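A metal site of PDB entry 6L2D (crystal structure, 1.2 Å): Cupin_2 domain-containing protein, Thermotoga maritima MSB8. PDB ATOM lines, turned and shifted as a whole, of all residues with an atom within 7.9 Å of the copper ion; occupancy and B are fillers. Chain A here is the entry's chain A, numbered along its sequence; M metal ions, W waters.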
ATOM      1  N   ARG A  43     -20.557  21.420  -2.785  1.00  0.00           N
ATOM      2  CA  ARG A  43     -20.656  19.979  -2.561  1.00  0.00           C
ATOM      3  C   ARG A  43     -21.928  19.678  -1.795  1.00  0.00           C
ATOM      4  O   ARG A  43     -22.426  20.503  -1.032  1.00  0.00           O
ATOM      5  CB  ARG A  43     -19.459  19.461  -1.763  1.00  0.00           C
ATOM      6  CG  ARG A  43     -18.108  19.685  -2.448  1.00  0.00           C
ATOM      7  CD  ARG A  43     -17.422  20.944  -2.000  1.00  0.00           C
ATOM      8  NE  ARG A  43     -17.235  21.132  -0.575  1.00  0.00           N
ATOM      9  CZ  ARG A  43     -16.291  20.574   0.164  1.00  0.00           C
ATOM     10  NH1 ARG A  43     -16.241  20.843   1.459  1.00  0.00           N
ATOM     11  NH2 ARG A  43     -15.387  19.760  -0.343  1.00  0.00           N
ATOM     12  N   ILE A  53     -17.809  13.092  10.963  1.00  0.00           N
ATOM     13  CA  ILE A  53     -16.712  13.943  10.537  1.00  0.00           C
ATOM     14  C   ILE A  53     -16.092  14.502  11.807  1.00  0.00           C
ATOM     15  O   ILE A  53     -16.672  15.402  12.395  1.00  0.00           O
ATOM     16  CB  ILE A  53     -17.213  15.045   9.600  1.00  0.00           C
ATOM     17  CG1 ILE A  53     -17.819  14.459   8.329  1.00  0.00           C
ATOM     18  CG2 ILE A  53     -16.123  16.056   9.275  1.00  0.00           C
ATOM     19  CD1 ILE A  53     -18.608  15.408   7.487  1.00  0.00           C
ATOM     20  N   ASP A  54     -14.978  13.902  12.258  1.00  0.00           N
ATOM     21  CA  ASP A  54     -14.453  14.241  13.564  1.00  0.00           C
ATOM     22  C   ASP A  54     -14.014  15.714  13.579  1.00  0.00           C
ATOM     23  O   ASP A  54     -13.736  16.328  12.543  1.00  0.00           O
ATOM     24  CB  ASP A  54     -13.395  13.281  14.083  1.00  0.00           C
ATOM     25  CG  ASP A  54     -13.532  13.068  15.583  1.00  0.00           C
ATOM     26  OD1 ASP A  54     -14.226  13.853  16.270  1.00  0.00           O
ATOM     27  OD2 ASP A  54     -12.927  12.099  16.096  1.00  0.00           O
ATOM     28  N   ARG A  55     -13.917  16.233  14.796  1.00  0.00           N
ATOM     29  CA  ARG A  55     -13.435  17.596  15.017  1.00  0.00           C
ATOM     30  C   ARG A  55     -12.119  17.822  14.289  1.00  0.00           C
ATOM     31  O   ARG A  55     -11.194  17.000  14.365  1.00  0.00           O
ATOM     32  CB  ARG A  55     -13.256  17.873  16.515  1.00  0.00           C
ATOM     33  CG  ARG A  55     -14.556  18.176  17.260  1.00  0.00           C
ATOM     34  CD  ARG A  55     -14.254  18.481  18.731  1.00  0.00           C
ATOM     35  NE  ARG A  55     -15.499  18.809  19.430  1.00  0.00           N
ATOM     36  CZ  ARG A  55     -16.355  17.935  19.930  1.00  0.00           C
ATOM     37  NH1 ARG A  55     -16.142  16.635  19.843  1.00  0.00           N
ATOM     38  NH2 ARG A  55     -17.436  18.414  20.535  1.00  0.00           N
ATOM     39  N   HIS A  56     -12.049  18.928  13.565  1.00  0.00           N
ATOM     40  CA  HIS A  56     -10.904  19.315  12.769  1.00  0.00           C
ATOM     41  C   HIS A  56     -10.951  20.814  12.553  1.00  0.00           C
ATOM     42  O   HIS A  56     -11.909  21.514  12.908  1.00  0.00           O
ATOM     43  CB  HIS A  56     -10.876  18.569  11.434  1.00  0.00           C
ATOM     44  CG  HIS A  56     -12.014  18.954  10.542  1.00  0.00           C
ATOM     45  ND1 HIS A  56     -13.296  18.484  10.679  1.00  0.00           N
ATOM     46  CD2 HIS A  56     -12.062  19.801   9.478  1.00  0.00           C
ATOM     47  CE1 HIS A  56     -14.074  19.018   9.726  1.00  0.00           C
ATOM     48  NE2 HIS A  56     -13.349  19.842   8.982  1.00  0.00           N
ATOM     49  N   SER A  57      -9.897  21.308  11.917  1.00  0.00           N
ATOM     50  CA  SER A  57      -9.891  22.707  11.482  1.00  0.00           C
ATOM     51  C   SER A  57      -9.005  22.827  10.253  1.00  0.00           C
ATOM     52  O   SER A  57      -8.173  21.961   9.973  1.00  0.00           O
ATOM     53  CB  SER A  57      -9.385  23.622  12.591  1.00  0.00           C
ATOM     54  OG  SER A  57      -8.045  23.289  12.959  1.00  0.00           O
ATOM     55  N   HIS A  58      -9.175  23.935   9.548  1.00  0.00           N
ATOM     56  CA  HIS A  58      -8.417  24.192   8.328  1.00  0.00           C
ATOM     57  C   HIS A  58      -8.425  25.691   8.066  1.00  0.00           C
ATOM     58  O   HIS A  58      -9.312  26.397   8.548  1.00  0.00           O
ATOM     59  CB  HIS A  58      -8.925  23.459   7.088  1.00  0.00           C
ATOM     60  CG  HIS A  58     -10.414  23.265   7.102  1.00  0.00           C
ATOM     61  ND1 HIS A  58     -11.336  24.288   7.108  1.00  0.00           N
ATOM     62  CD2 HIS A  58     -11.161  22.139   7.207  1.00  0.00           C
ATOM     63  CE1 HIS A  58     -12.566  23.781   7.158  1.00  0.00           C
ATOM     64  NE2 HIS A  58     -12.499  22.454   7.222  1.00  0.00           N
ATOM     65  N   TRP A  60      -9.483  27.711   5.920  1.00  0.00           N
ATOM     66  CA  TRP A  60     -10.565  28.244   5.142  1.00  0.00           C
ATOM     67  C   TRP A  60     -11.891  28.011   5.901  1.00  0.00           C
ATOM     68  O   TRP A  60     -11.982  27.131   6.753  1.00  0.00           O
ATOM     69  CB  TRP A  60     -10.675  27.618   3.755  1.00  0.00           C
ATOM     70  CG  TRP A  60     -10.836  26.115   3.741  1.00  0.00           C
ATOM     71  CD1 TRP A  60     -11.984  25.389   3.848  1.00  0.00           C
ATOM     72  CD2 TRP A  60      -9.755  25.189   3.596  1.00  0.00           C
ATOM     73  NE1 TRP A  60     -11.683  24.043   3.782  1.00  0.00           N
ATOM     74  CE2 TRP A  60     -10.331  23.900   3.623  1.00  0.00           C
ATOM     75  CE3 TRP A  60      -8.374  25.340   3.436  1.00  0.00           C
ATOM     76  CZ2 TRP A  60      -9.541  22.741   3.503  1.00  0.00           C
ATOM     77  CZ3 TRP A  60      -7.606  24.187   3.323  1.00  0.00           C
ATOM     78  CH2 TRP A  60      -8.197  22.926   3.351  1.00  0.00           C
ATOM     79  N   GLU A  61     -12.867  28.826   5.530  1.00  0.00           N
ATOM     80  CA  GLU A  61     -14.209  28.778   6.093  1.00  0.00           C
ATOM     81  C   GLU A  61     -15.063  27.694   5.449  1.00  0.00           C
ATOM     82  O   GLU A  61     -14.747  27.219   4.348  1.00  0.00           O
ATOM     83  CB  GLU A  61     -14.912  30.119   5.880  1.00  0.00           C
ATOM     84  CG  GLU A  61     -15.239  30.481   4.431  1.00  0.00           C
ATOM     85  CD  GLU A  61     -14.160  31.103   3.581  1.00  0.00           C
ATOM     86  OE1 GLU A  61     -12.969  31.017   3.954  1.00  0.00           O
ATOM     87  OE2 GLU A  61     -14.482  31.707   2.531  1.00  0.00           O
ATOM     88  N   HIS A  62     -16.150  27.349   6.123  1.00  0.00           N
ATOM     89  CA  HIS A  62     -17.252  26.615   5.545  1.00  0.00           C
ATOM     90  C   HIS A  62     -18.530  27.476   5.548  1.00  0.00           C
ATOM     91  O   HIS A  62     -18.807  28.156   6.525  1.00  0.00           O
ATOM     92  CB  HIS A  62     -17.648  25.348   6.279  1.00  0.00           C
ATOM     93  CG  HIS A  62     -16.764  24.156   6.280  1.00  0.00           C
ATOM     94  ND1 HIS A  62     -16.571  23.335   5.203  1.00  0.00           N
ATOM     95  CD2 HIS A  62     -16.064  23.584   7.296  1.00  0.00           C
ATOM     96  CE1 HIS A  62     -15.768  22.345   5.530  1.00  0.00           C
ATOM     97  NE2 HIS A  62     -15.437  22.459   6.827  1.00  0.00           N
ATOM     98  N   ILE A  64     -22.517  26.333   5.066  1.00  0.00           N
ATOM     99  CA  ILE A  64     -23.294  25.093   5.039  1.00  0.00           C
ATOM    100  C   ILE A  64     -24.777  25.387   5.088  1.00  0.00           C
ATOM    101  O   ILE A  64     -25.200  26.323   5.783  1.00  0.00           O
ATOM    102  CB  ILE A  64     -22.886  24.166   6.200  1.00  0.00           C
ATOM    103  CG1 ILE A  64     -21.509  23.575   5.914  1.00  0.00           C
ATOM    104  CG2 ILE A  64     -23.876  23.055   6.479  1.00  0.00           C
ATOM    105  CD1 ILE A  64     -20.809  22.993   7.116  1.00  0.00           C
ATOM    106  N   VAL A  90     -18.760  28.514   9.502  1.00  0.00           N
ATOM    107  CA  VAL A  90     -17.596  28.119  10.272  1.00  0.00           C
ATOM    108  C   VAL A  90     -16.447  29.028   9.852  1.00  0.00           C
ATOM    109  O   VAL A  90     -16.044  29.000   8.696  1.00  0.00           O
ATOM    110  CB  VAL A  90     -17.186  26.657  10.077  1.00  0.00           C
ATOM    111  CG1 VAL A  90     -16.092  26.278  11.050  1.00  0.00           C
ATOM    112  CG2 VAL A  90     -18.379  25.722  10.302  1.00  0.00           C
ATOM    113  N   GLU A  94     -11.576  27.550  12.934  1.00  0.00           N
ATOM    114  CA  GLU A  94     -12.448  27.153  14.054  1.00  0.00           C
ATOM    115  C   GLU A  94     -12.582  25.645  14.077  1.00  0.00           C
ATOM    116  O   GLU A  94     -12.791  25.009  13.040  1.00  0.00           O
ATOM    117  CB  GLU A  94     -13.791  27.830  13.843  1.00  0.00           C
ATOM    118  CG  GLU A  94     -14.899  27.681  14.842  1.00  0.00           C
ATOM    119  CD  GLU A  94     -16.101  28.599  14.726  1.00  0.00           C
ATOM    120  OE1 GLU A  94     -16.478  29.228  13.709  1.00  0.00           O
ATOM    121  OE2 GLU A  94     -16.775  28.699  15.782  1.00  0.00           O
ATOM    122  N   ILE A  95     -12.498  25.060  15.265  1.00  0.00           N
ATOM    123  CA  ILE A  95     -12.678  23.626  15.432  1.00  0.00           C
ATOM    124  C   ILE A  95     -14.141  23.275  15.193  1.00  0.00           C
ATOM    125  O   ILE A  95     -15.051  23.937  15.694  1.00  0.00           O
ATOM    126  CB  ILE A  95     -12.221  23.192  16.835  1.00  0.00           C
ATOM    127  CG1 ILE A  95     -10.687  23.310  16.989  1.00  0.00           C
ATOM    128  CG2 ILE A  95     -12.689  21.786  17.191  1.00  0.00           C
ATOM    129  CD1 ILE A  95     -10.346  23.340  18.467  1.00  0.00           C
ATOM    130  N   HIS A  96     -14.401  22.245  14.399  1.00  0.00           N
ATOM    131  CA  HIS A  96     -15.759  21.848  14.064  1.00  0.00           C
ATOM    132  C   HIS A  96     -15.766  20.394  13.616  1.00  0.00           C
ATOM    133  O   HIS A  96     -14.756  19.870  13.135  1.00  0.00           O
ATOM    134  CB  HIS A  96     -16.348  22.724  12.946  1.00  0.00           C
ATOM    135  CG  HIS A  96     -15.569  22.633  11.664  1.00  0.00           C
ATOM    136  ND1 HIS A  96     -14.346  23.228  11.542  1.00  0.00           N
ATOM    137  CD2 HIS A  96     -15.794  22.004  10.494  1.00  0.00           C
ATOM    138  CE1 HIS A  96     -13.887  22.976  10.315  1.00  0.00           C
ATOM    139  NE2 HIS A  96     -14.725  22.234   9.660  1.00  0.00           N
ATOM    140  N   GLY A  97     -16.902  19.734  13.720  1.00  0.00           N
ATOM    141  CA  GLY A  97     -17.130  18.432  13.137  1.00  0.00           C
ATOM    142  C   GLY A  97     -18.627  18.171  13.052  1.00  0.00           C
ATOM    143  O   GLY A  97     -19.407  19.055  13.442  1.00  0.00           O
ATOM    144  N   PHE A  98     -19.029  17.009  12.544  1.00  0.00           N
ATOM    145  CA  PHE A  98     -20.426  16.672  12.335  1.00  0.00           C
ATOM    146  C   PHE A  98     -20.692  15.206  12.652  1.00  0.00           C
ATOM    147  O   PHE A  98     -19.827  14.354  12.440  1.00  0.00           O
ATOM    148  CB  PHE A  98     -20.825  16.973  10.889  1.00  0.00           C
ATOM    149  CG  PHE A  98     -20.487  18.392  10.514  1.00  0.00           C
ATOM    150  CD1 PHE A  98     -21.310  19.431  10.933  1.00  0.00           C
ATOM    151  CD2 PHE A  98     -19.355  18.668   9.760  1.00  0.00           C
ATOM    152  CE1 PHE A  98     -20.963  20.727  10.566  1.00  0.00           C
ATOM    153  CE2 PHE A  98     -19.012  19.955   9.402  1.00  0.00           C
ATOM    154  CZ  PHE A  98     -19.825  20.988   9.830  1.00  0.00           C
ATOM    155  N   CSD A 110     -22.321  22.174   1.303  1.00  0.00           N
ATOM    156  CA  CSD A 110     -21.087  22.674   1.954  1.00  0.00           C
ATOM    157  CB  CSD A 110     -20.333  21.497   2.540  1.00  0.00           C
ATOM    158  SG  CSD A 110     -18.945  22.047   3.507  1.00  0.00           S
ATOM    159  C   CSD A 110     -20.244  23.338   0.836  1.00  0.00           C
ATOM    160  O   CSD A 110     -19.947  22.709  -0.176  1.00  0.00           O
ATOM    161  OD1 CSD A 110     -18.353  20.680   4.059  1.00  0.00           O
ATOM    162  OD2 CSD A 110     -18.011  22.509   2.506  1.00  0.00           O
ATOM    163  N   ILE A 112     -16.872  25.895   0.115  1.00  0.00           N
ATOM    164  CA  ILE A 112     -15.573  26.346   0.571  1.00  0.00           C
ATOM    165  C   ILE A 112     -14.910  27.143  -0.543  1.00  0.00           C
ATOM    166  O   ILE A 112     -15.185  26.877  -1.740  1.00  0.00           O
ATOM    167  CB  ILE A 112     -14.657  25.192   1.019  1.00  0.00           C
ATOM    168  CG1 ILE A 112     -14.334  24.190  -0.078  1.00  0.00           C
ATOM    169  CG2 ILE A 112     -15.238  24.461   2.230  1.00  0.00           C
ATOM    170  CD1 ILE A 112     -13.326  23.110   0.305  1.00  0.00           C
HETATM  171 CU    CU M   1     -14.206  21.328   7.875  1.00  0.00          CU
HETATM  172  O   HOH W   1     -14.170  20.066   6.504  1.00  0.00           O
HETATM  173  O   HOH W   2     -16.168  19.413   7.528  1.00  0.00           O
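The copper ion is bound by water W1, NE2 of His 62, NE2 of His 56, NE2 of His 96 and NE2 of His 58. The copper ion has five donor atoms within binding distance. Slightly farther from the copper ion lies water W2 (2.8 Å).
Within 4 Å of the copper ion: His 56, His 58, His 62 and His 96. Along chain A the residues within 4 Å of the copper ion span positions 56 to 96. The nearest printed residue that does not touch the copper ion is Phe 98 (5.2 Å).
A ring nitrogen (ND1) of His 96 lies within hydrogen-bond range of the backbone carbonyl oxygen of Glu 94, at 2.8 Å. A ring nitrogen (ND1) of His 58 is in hydrogen-bond range of the backbone carbonyl oxygen (O) of Trp 60, 2.9 Å away. ND1 of His 56 is in hydrogen-bond range of O of Asp 54 (2.9 Å). O of His 62 lies within hydrogen-bond range of N of Val 90, at 3.0 Å. ND1 of His 62 is in hydrogen-bond range of OD2 of CSD 110 (3.2 Å).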
